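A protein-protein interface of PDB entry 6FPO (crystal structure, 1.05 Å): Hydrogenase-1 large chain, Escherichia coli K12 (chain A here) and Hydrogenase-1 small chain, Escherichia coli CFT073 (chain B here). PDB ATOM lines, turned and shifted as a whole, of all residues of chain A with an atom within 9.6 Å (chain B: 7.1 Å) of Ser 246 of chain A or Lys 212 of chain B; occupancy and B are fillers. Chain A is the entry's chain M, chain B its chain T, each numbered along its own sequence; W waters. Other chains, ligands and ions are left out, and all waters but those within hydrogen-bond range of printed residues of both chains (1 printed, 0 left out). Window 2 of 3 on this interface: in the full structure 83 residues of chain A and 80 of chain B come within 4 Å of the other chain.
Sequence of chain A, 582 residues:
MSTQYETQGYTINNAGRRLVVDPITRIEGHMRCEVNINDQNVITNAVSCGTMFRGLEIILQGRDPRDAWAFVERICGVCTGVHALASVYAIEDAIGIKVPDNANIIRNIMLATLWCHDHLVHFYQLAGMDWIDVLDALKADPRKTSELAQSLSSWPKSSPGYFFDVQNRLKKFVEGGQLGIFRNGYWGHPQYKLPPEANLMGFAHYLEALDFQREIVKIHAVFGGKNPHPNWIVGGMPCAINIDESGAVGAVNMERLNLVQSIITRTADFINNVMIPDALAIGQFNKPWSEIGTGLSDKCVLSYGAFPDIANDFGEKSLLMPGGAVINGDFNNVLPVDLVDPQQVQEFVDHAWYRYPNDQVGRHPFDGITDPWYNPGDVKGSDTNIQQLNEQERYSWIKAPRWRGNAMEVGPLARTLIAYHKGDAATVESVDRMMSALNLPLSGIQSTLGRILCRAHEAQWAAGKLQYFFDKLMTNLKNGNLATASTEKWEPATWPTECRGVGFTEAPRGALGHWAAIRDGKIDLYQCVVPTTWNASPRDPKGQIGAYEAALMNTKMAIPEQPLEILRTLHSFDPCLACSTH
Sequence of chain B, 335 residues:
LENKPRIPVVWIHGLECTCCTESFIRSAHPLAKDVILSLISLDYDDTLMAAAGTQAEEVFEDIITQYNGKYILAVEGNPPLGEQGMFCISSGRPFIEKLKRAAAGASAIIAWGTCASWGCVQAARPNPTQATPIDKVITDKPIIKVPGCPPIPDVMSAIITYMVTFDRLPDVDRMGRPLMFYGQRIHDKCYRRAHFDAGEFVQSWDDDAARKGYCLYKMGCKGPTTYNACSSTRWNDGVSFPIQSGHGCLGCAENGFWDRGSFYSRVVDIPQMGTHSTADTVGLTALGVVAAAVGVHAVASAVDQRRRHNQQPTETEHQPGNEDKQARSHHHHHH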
ATOM      1  N   PRO A 238     -17.742 -28.860  13.506  1.00  0.00           N
ATOM      2  CA  PRO A 238     -18.723 -27.859  13.047  1.00  0.00           C
ATOM      3  C   PRO A 238     -18.158 -26.454  12.941  1.00  0.00           C
ATOM      4  O   PRO A 238     -18.830 -25.537  12.497  1.00  0.00           O
ATOM      5  CB  PRO A 238     -19.830 -27.940  14.053  1.00  0.00           C
ATOM      6  CG  PRO A 238     -19.246 -28.570  15.239  1.00  0.00           C
ATOM      7  CD  PRO A 238     -17.974 -29.231  14.910  1.00  0.00           C
ATOM      8  N   CYS A 239     -16.913 -26.272  13.383  1.00  0.00           N
ATOM      9  CA  CYS A 239     -16.266 -24.954  13.428  1.00  0.00           C
ATOM     10  C   CYS A 239     -15.693 -24.588  12.048  1.00  0.00           C
ATOM     11  O   CYS A 239     -14.478 -24.578  11.828  1.00  0.00           O
ATOM     12  CB  CYS A 239     -15.228 -24.947  14.543  1.00  0.00           C
ATOM     13  SG  CYS A 239     -13.999 -26.273  14.468  1.00  0.00           S
ATOM     14  N   ALA A 240     -16.588 -24.203  11.162  1.00  0.00           N
ATOM     15  CA  ALA A 240     -16.230 -23.792   9.825  1.00  0.00           C
ATOM     16  C   ALA A 240     -15.193 -22.645   9.909  1.00  0.00           C
ATOM     17  O   ALA A 240     -15.263 -21.786  10.782  1.00  0.00           O
ATOM     18  CB  ALA A 240     -17.469 -23.346   9.086  1.00  0.00           C
ATOM     19  N   ILE A 241     -14.307 -22.647   8.921  1.00  0.00           N
ATOM     20  CA  ILE A 241     -13.188 -21.692   8.847  1.00  0.00           C
ATOM     21  C   ILE A 241     -13.410 -20.705   7.726  1.00  0.00           C
ATOM     22  O   ILE A 241     -13.852 -21.074   6.623  1.00  0.00           O
ATOM     23  CB  ILE A 241     -11.866 -22.444   8.638  1.00  0.00           C
ATOM     24  CG1 ILE A 241     -11.601 -23.389   9.798  1.00  0.00           C
ATOM     25  CG2 ILE A 241     -10.688 -21.476   8.438  1.00  0.00           C
ATOM     26  CD1 ILE A 241     -10.435 -24.348   9.568  1.00  0.00           C
ATOM     27  N   ASN A 242     -13.119 -19.440   8.003  1.00  0.00           N
ATOM     28  CA  ASN A 242     -13.157 -18.378   6.992  1.00  0.00           C
ATOM     29  C   ASN A 242     -12.121 -17.359   7.423  1.00  0.00           C
ATOM     30  O   ASN A 242     -12.280 -16.726   8.467  1.00  0.00           O
ATOM     31  CB  ASN A 242     -14.560 -17.777   6.906  1.00  0.00           C
ATOM     32  CG  ASN A 242     -14.660 -16.668   5.936  1.00  0.00           C
ATOM     33  OD1 ASN A 242     -13.677 -16.170   5.392  1.00  0.00           O
ATOM     34  ND2 ASN A 242     -15.888 -16.210   5.703  1.00  0.00           N
ATOM     35  N   ILE A 243     -11.026 -17.268   6.669  1.00  0.00           N
ATOM     36  CA  ILE A 243      -9.951 -16.333   7.008  1.00  0.00           C
ATOM     37  C   ILE A 243     -10.040 -15.011   6.260  1.00  0.00           C
ATOM     38  O   ILE A 243      -9.767 -13.985   6.830  1.00  0.00           O
ATOM     39  CB  ILE A 243      -8.559 -16.987   6.793  1.00  0.00           C
ATOM     40  CG1 ILE A 243      -8.405 -18.367   7.345  1.00  0.00           C
ATOM     41  CG2 ILE A 243      -7.461 -16.023   7.204  1.00  0.00           C
ATOM     42  CD1 ILE A 243      -8.684 -18.337   8.803  1.00  0.00           C
ATOM     43  N   ASP A 244     -10.429 -15.045   4.978  1.00  0.00           N
ATOM     44  CA  ASP A 244     -10.203 -13.880   4.100  1.00  0.00           C
ATOM     45  C   ASP A 244     -11.410 -13.551   3.246  1.00  0.00           C
ATOM     46  O   ASP A 244     -11.254 -12.860   2.255  1.00  0.00           O
ATOM     47  CB  ASP A 244      -8.986 -14.096   3.227  1.00  0.00           C
ATOM     48  CG  ASP A 244      -8.481 -12.867   2.480  1.00  0.00           C
ATOM     49  OD1 ASP A 244      -8.455 -11.773   3.052  1.00  0.00           O
ATOM     50  OD2 ASP A 244      -8.065 -13.035   1.288  1.00  0.00           O
ATOM     51  N   GLU A 245     -12.601 -14.002   3.628  1.00  0.00           N
ATOM     52  CA  GLU A 245     -13.815 -13.742   2.893  1.00  0.00           C
ATOM     53  C   GLU A 245     -14.803 -12.978   3.769  1.00  0.00           C
ATOM     54  O   GLU A 245     -14.709 -12.943   4.995  1.00  0.00           O
ATOM     55  CB  GLU A 245     -14.396 -15.069   2.374  1.00  0.00           C
ATOM     56  CG  GLU A 245     -13.387 -15.937   1.582  1.00  0.00           C
ATOM     57  CD  GLU A 245     -13.741 -17.426   1.509  1.00  0.00           C
ATOM     58  OE1 GLU A 245     -14.646 -17.692   0.729  1.00  0.00           O
ATOM     59  OE2 GLU A 245     -13.147 -18.287   2.256  1.00  0.00           O
ATOM     60  N   SER A 246     -15.801 -12.385   3.113  1.00  0.00           N
ATOM     61  CA  SER A 246     -16.848 -11.732   3.847  1.00  0.00           C
ATOM     62  C   SER A 246     -17.481 -12.743   4.802  1.00  0.00           C
ATOM     63  O   SER A 246     -17.651 -13.911   4.494  1.00  0.00           O
ATOM     64  CB  SER A 246     -17.877 -11.225   2.830  1.00  0.00           C
ATOM     65  OG  SER A 246     -18.886 -10.526   3.479  1.00  0.00           O
ATOM     66  N   GLY A 247     -17.843 -12.242   5.971  1.00  0.00           N
ATOM     67  CA  GLY A 247     -18.481 -13.109   6.947  1.00  0.00           C
ATOM     68  C   GLY A 247     -17.526 -13.915   7.790  1.00  0.00           C
ATOM     69  O   GLY A 247     -17.978 -14.766   8.561  1.00  0.00           O
ATOM     70  N   ALA A 248     -16.220 -13.610   7.746  1.00  0.00           N
ATOM     71  CA  ALA A 248     -15.273 -14.299   8.619  1.00  0.00           C
ATOM     72  C   ALA A 248     -15.619 -14.062  10.077  1.00  0.00           C
ATOM     73  O   ALA A 248     -15.231 -14.883  10.925  1.00  0.00           O
ATOM     74  CB  ALA A 248     -13.873 -13.910   8.291  1.00  0.00           C
ATOM     75  N   VAL A 249     -16.307 -12.991  10.406  1.00  0.00           N
ATOM     76  CA  VAL A 249     -16.803 -12.754  11.750  1.00  0.00           C
ATOM     77  C   VAL A 249     -17.733 -13.852  12.249  1.00  0.00           C
ATOM     78  O   VAL A 249     -17.947 -13.928  13.464  1.00  0.00           O
ATOM     79  CB  VAL A 249     -17.534 -11.385  11.862  1.00  0.00           C
ATOM     80  CG1 VAL A 249     -16.550 -10.237  11.671  1.00  0.00           C
ATOM     81  CG2 VAL A 249     -18.733 -11.279  10.915  1.00  0.00           C
ATOM     82  N   GLY A 250     -18.267 -14.661  11.348  1.00  0.00           N
ATOM     83  CA  GLY A 250     -19.121 -15.786  11.692  1.00  0.00           C
ATOM     84  C   GLY A 250     -18.454 -17.131  11.748  1.00  0.00           C
ATOM     85  O   GLY A 250     -19.153 -18.146  11.734  1.00  0.00           O
ATOM     86  N   ALA A 251     -17.126 -17.159  11.802  1.00  0.00           N
ATOM     87  CA  ALA A 251     -16.390 -18.399  11.606  1.00  0.00           C
ATOM     88  C   ALA A 251     -15.058 -18.378  12.372  1.00  0.00           C
ATOM     89  O   ALA A 251     -14.703 -17.395  13.021  1.00  0.00           O
ATOM     90  CB  ALA A 251     -16.138 -18.605  10.128  1.00  0.00           C
ATOM     91  N   VAL A 252     -14.314 -19.482  12.273  1.00  0.00           N
ATOM     92  CA  VAL A 252     -12.947 -19.491  12.789  1.00  0.00           C
ATOM     93  C   VAL A 252     -12.103 -18.649  11.857  1.00  0.00           C
ATOM     94  O   VAL A 252     -11.878 -19.043  10.710  1.00  0.00           O
ATOM     95  CB  VAL A 252     -12.414 -20.914  12.924  1.00  0.00           C
ATOM     96  CG1 VAL A 252     -10.938 -20.892  13.295  1.00  0.00           C
ATOM     97  CG2 VAL A 252     -13.206 -21.735  13.937  1.00  0.00           C
ATOM     98  N   ASN A 253     -11.653 -17.494  12.341  1.00  0.00           N
ATOM     99  CA  ASN A 253     -10.962 -16.489  11.541  1.00  0.00           C
ATOM    100  C   ASN A 253      -9.578 -16.250  12.176  1.00  0.00           C
ATOM    101  O   ASN A 253      -9.172 -16.961  13.103  1.00  0.00           O
ATOM    102  CB  ASN A 253     -11.800 -15.221  11.462  1.00  0.00           C
ATOM    103  CG  ASN A 253     -12.088 -14.632  12.816  1.00  0.00           C
ATOM    104  OD1 ASN A 253     -11.178 -14.521  13.652  1.00  0.00           O
ATOM    105  ND2 ASN A 253     -13.306 -14.220  13.076  1.00  0.00           N
ATOM    106  N   ARG B 192     -26.901 -14.694  15.829  1.00  0.00           N
ATOM    107  CA  ARG B 192     -27.271 -15.130  14.490  1.00  0.00           C
ATOM    108  C   ARG B 192     -28.734 -14.915  14.187  1.00  0.00           C
ATOM    109  O   ARG B 192     -29.222 -15.345  13.117  1.00  0.00           O
ATOM    110  CB  ARG B 192     -26.868 -16.608  14.235  1.00  0.00           C
ATOM    111  CG  ARG B 192     -25.388 -16.823  14.381  1.00  0.00           C
ATOM    112  CD  ARG B 192     -24.944 -18.203  13.977  1.00  0.00           C
ATOM    113  NE  ARG B 192     -23.496 -18.359  14.210  1.00  0.00           N
ATOM    114  CZ  ARG B 192     -22.731 -19.270  13.628  1.00  0.00           C
ATOM    115  NH1 ARG B 192     -23.206 -20.120  12.738  1.00  0.00           N
ATOM    116  NH2 ARG B 192     -21.445 -19.292  13.936  1.00  0.00           N
ATOM    117  N   HIS B 195     -29.890 -13.661  10.779  1.00  0.00           N
ATOM    118  CA  HIS B 195     -29.941 -14.685   9.734  1.00  0.00           C
ATOM    119  C   HIS B 195     -31.213 -15.500   9.813  1.00  0.00           C
ATOM    120  O   HIS B 195     -31.874 -15.767   8.809  1.00  0.00           O
ATOM    121  CB  HIS B 195     -28.712 -15.556   9.784  1.00  0.00           C
ATOM    122  CG  HIS B 195     -27.435 -14.798   9.607  1.00  0.00           C
ATOM    123  ND1 HIS B 195     -27.200 -13.988   8.509  1.00  0.00           N
ATOM    124  CD2 HIS B 195     -26.342 -14.690  10.384  1.00  0.00           C
ATOM    125  CE1 HIS B 195     -25.991 -13.444   8.661  1.00  0.00           C
ATOM    126  NE2 HIS B 195     -25.439 -13.876   9.774  1.00  0.00           N
ATOM    127  N   VAL B 202     -27.601 -22.337   7.521  1.00  0.00           N
ATOM    128  CA  VAL B 202     -26.771 -23.492   7.196  1.00  0.00           C
ATOM    129  C   VAL B 202     -27.663 -24.633   6.799  1.00  0.00           C
ATOM    130  O   VAL B 202     -28.604 -24.980   7.491  1.00  0.00           O
ATOM    131  CB  VAL B 202     -25.878 -23.863   8.407  1.00  0.00           C
ATOM    132  CG1 VAL B 202     -25.041 -25.064   8.091  1.00  0.00           C
ATOM    133  CG2 VAL B 202     -25.021 -22.673   8.808  1.00  0.00           C
ATOM    134  N   ASP B 207     -20.945 -25.647   4.511  1.00  0.00           N
ATOM    135  CA  ASP B 207     -21.395 -24.976   3.327  1.00  0.00           C
ATOM    136  C   ASP B 207     -21.043 -23.515   3.372  1.00  0.00           C
ATOM    137  O   ASP B 207     -20.471 -23.000   4.349  1.00  0.00           O
ATOM    138  CB  ASP B 207     -22.879 -25.278   3.052  1.00  0.00           C
ATOM    139  CG  ASP B 207     -23.876 -24.710   4.019  1.00  0.00           C
ATOM    140  OD1 ASP B 207     -23.505 -23.966   4.928  1.00  0.00           O
ATOM    141  OD2 ASP B 207     -25.091 -25.074   3.844  1.00  0.00           O
ATOM    142  N   ASP B 208     -21.369 -22.758   2.308  1.00  0.00           N
ATOM    143  CA  ASP B 208     -21.005 -21.357   2.287  1.00  0.00           C
ATOM    144  C   ASP B 208     -21.705 -20.579   3.410  1.00  0.00           C
ATOM    145  O   ASP B 208     -21.093 -19.680   4.019  1.00  0.00           O
ATOM    146  CB  ASP B 208     -21.246 -20.739   0.943  1.00  0.00           C
ATOM    147  CG  ASP B 208     -20.273 -21.237  -0.138  1.00  0.00           C
ATOM    148  OD1 ASP B 208     -19.210 -21.865   0.176  1.00  0.00           O
ATOM    149  OD2 ASP B 208     -20.526 -20.868  -1.292  1.00  0.00           O
ATOM    150  N   ALA B 209     -22.944 -20.945   3.722  1.00  0.00           N
ATOM    151  CA  ALA B 209     -23.682 -20.343   4.813  1.00  0.00           C
ATOM    152  C   ALA B 209     -22.953 -20.553   6.137  1.00  0.00           C
ATOM    153  O   ALA B 209     -22.850 -19.647   6.962  1.00  0.00           O
ATOM    154  CB  ALA B 209     -25.042 -20.948   4.853  1.00  0.00           C
ATOM    155  N   ALA B 210     -22.478 -21.781   6.370  1.00  0.00           N
ATOM    156  CA  ALA B 210     -21.760 -22.062   7.631  1.00  0.00           C
ATOM    157  C   ALA B 210     -20.507 -21.192   7.749  1.00  0.00           C
ATOM    158  O   ALA B 210     -20.188 -20.720   8.850  1.00  0.00           O
ATOM    159  CB  ALA B 210     -21.358 -23.536   7.664  1.00  0.00           C
ATOM    160  N   ARG B 211     -19.818 -20.973   6.635  1.00  0.00           N
ATOM    161  CA  ARG B 211     -18.579 -20.167   6.629  1.00  0.00           C
ATOM    162  C   ARG B 211     -18.823 -18.665   6.811  1.00  0.00           C
ATOM    163  O   ARG B 211     -17.882 -17.948   7.021  1.00  0.00           O
ATOM    164  CB  ARG B 211     -17.801 -20.450   5.358  1.00  0.00           C
ATOM    165  CG  ARG B 211     -17.218 -21.871   5.311  1.00  0.00           C
ATOM    166  CD  ARG B 211     -16.615 -22.209   3.943  1.00  0.00           C
ATOM    167  NE  ARG B 211     -16.104 -23.559   3.888  1.00  0.00           N
ATOM    168  CZ  ARG B 211     -15.304 -24.019   2.962  1.00  0.00           C
ATOM    169  NH1 ARG B 211     -14.939 -23.295   1.942  1.00  0.00           N
ATOM    170  NH2 ARG B 211     -14.860 -25.254   3.076  1.00  0.00           N
ATOM    171  N   LYS B 212     -20.099 -18.251   6.754  1.00  0.00           N
ATOM    172  CA  LYS B 212     -20.492 -16.856   7.026  1.00  0.00           C
ATOM    173  C   LYS B 212     -21.234 -16.714   8.334  1.00  0.00           C
ATOM    174  O   LYS B 212     -21.725 -15.617   8.645  1.00  0.00           O
ATOM    175  CB  LYS B 212     -21.431 -16.362   5.866  1.00  0.00           C
ATOM    176  CG  LYS B 212     -20.816 -16.208   4.531  1.00  0.00           C
ATOM    177  CD  LYS B 212     -21.884 -15.846   3.495  1.00  0.00           C
ATOM    178  CE  LYS B 212     -22.800 -16.874   2.993  1.00  0.00           C
ATOM    179  NZ  LYS B 212     -23.456 -16.280   1.790  1.00  0.00           N
ATOM    180  N   GLY B 213     -21.344 -17.789   9.105  1.00  0.00           N
ATOM    181  CA  GLY B 213     -22.028 -17.737  10.401  1.00  0.00           C
ATOM    182  C   GLY B 213     -23.548 -17.596  10.322  1.00  0.00           C
ATOM    183  O   GLY B 213     -24.146 -16.979  11.182  1.00  0.00           O
ATOM    184  N   TYR B 214     -24.176 -18.250   9.326  1.00  0.00           N
ATOM    185  CA  TYR B 214     -25.632 -18.239   9.249  1.00  0.00           C
ATOM    186  C   TYR B 214     -26.257 -19.070  10.343  1.00  0.00           C
ATOM    187  O   TYR B 214     -25.623 -19.802  11.108  1.00  0.00           O
ATOM    188  CB  TYR B 214     -26.100 -18.685   7.851  1.00  0.00           C
ATOM    189  CG  TYR B 214     -25.911 -17.643   6.739  1.00  0.00           C
ATOM    190  CD1 TYR B 214     -25.270 -16.433   6.919  1.00  0.00           C
ATOM    191  CD2 TYR B 214     -26.469 -17.885   5.488  1.00  0.00           C
ATOM    192  CE1 TYR B 214     -25.135 -15.542   5.876  1.00  0.00           C
ATOM    193  CE2 TYR B 214     -26.343 -16.987   4.463  1.00  0.00           C
ATOM    194  CZ  TYR B 214     -25.696 -15.806   4.666  1.00  0.00           C
ATOM    195  OH  TYR B 214     -25.539 -14.883   3.622  1.00  0.00           O
ATOM    196  N   CYS B 215     -27.568 -18.880  10.497  1.00  0.00           N
ATOM    197  CA  CYS B 215     -28.323 -19.535  11.574  1.00  0.00           C
ATOM    198  C   CYS B 215     -28.318 -21.041  11.412  1.00  0.00           C
ATOM    199  O   CYS B 215     -28.343 -21.595  10.305  1.00  0.00           O
ATOM    200  CB  CYS B 215     -29.765 -18.953  11.546  1.00  0.00           C
ATOM    201  SG  CYS B 215     -30.962 -19.822  12.606  1.00  0.00           S
HETATM  202  O   HOH W   1     -19.316 -20.753  12.580  1.00  0.00           O
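Of the printed residues of chain B, Ala 240 of chain A touches Ala 210 (3.8 Å). Of the printed residues of chain B, Ile 241 of chain A touches Arg 211 (3.7 Å). Ile 243 of chain A touches none of the printed residues of chain B. Of the printed residues of chain B, Ala 251 of chain A touches Arg 211 (3.6 Å). No residue of chain A comes within 4 Å of Ala 209 of chain B. Of the printed residues of chain A, Arg 211 of chain B touches Ile 241, Asn 242, Gly 247 and Ala 251. Gly 213 of chain B touches one residue of chain A. The nearest printed residue of chain A that does not touch Lys 212 of chain B is Gly 250 of chain A (4.01 Å).
The guanidinium group (NH1) of Arg 192 of chain B sits at hydrogen-bond distance from the backbone carbonyl oxygen (O) of Tyr 214 of chain B, at 2.9 Å. OD1 of Asp 207 of chain B sits at hydrogen-bond distance from N of Ala 210 of chain B. O of Ala 240 of chain A lies within hydrogen-bond range of N of Val 252 of chain A (2.9 Å). The side-chain amide nitrogen of Asn 242 of chain A lies within hydrogen-bond range of the backbone carbonyl oxygen of Ser 246 of chain A (3.1 Å). The backbone NH (N) of Asn 242 of chain A sits at hydrogen-bond distance from the backbone carbonyl oxygen (O) of Val 252 of chain A, at 3.0 Å. The side-chain amide nitrogen (ND2) of Asn 253 of chain A sits at hydrogen-bond distance from the backbone carbonyl oxygen (O) of Ala 251 of chain A (3.5 Å).
Water W1 bridges O of Gly 250 of chain A and NH2 of Arg 192 of chain B.
The backbone carbonyl oxygen of Gly 250 of chain A lies within hydrogen-bond range of the guanidinium group of Arg 192 of chain B (3.4 Å). The side-chain amide nitrogen (ND2) of Asn 242 of chain A lies within hydrogen-bond range of the backbone carbonyl oxygen (O) of Arg 211 of chain B (3.0 Å). The backbone NH (N) of Gly 213 of chain B sits close to the backbone carbonyl oxygen (O) of Gly 250 of chain A, at 3.4 Å.
Among the printed residues, merely in contact across the chains: Ala 240 of chain A with Ala 210 of chain B (3.8 Å), Ile 241 of chain A with Arg 211 of chain B (3.7 Å), Ser 246 of chain A with Lys 212 of chain B (3.9 Å), Gly 247 of chain A with Arg 211 of chain B (3.5 Å), Gly 247 of chain A with Lys 212 of chain B (3.6 Å) and Ala 251 of chain A with Arg 211 of chain B (3.6 Å).
Hydrophobic or aromatic side chains of chain A that line the printed part of chain B: Ala 240 and Ala 251. Among the printed residues, 9 pairs touch across the chains.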
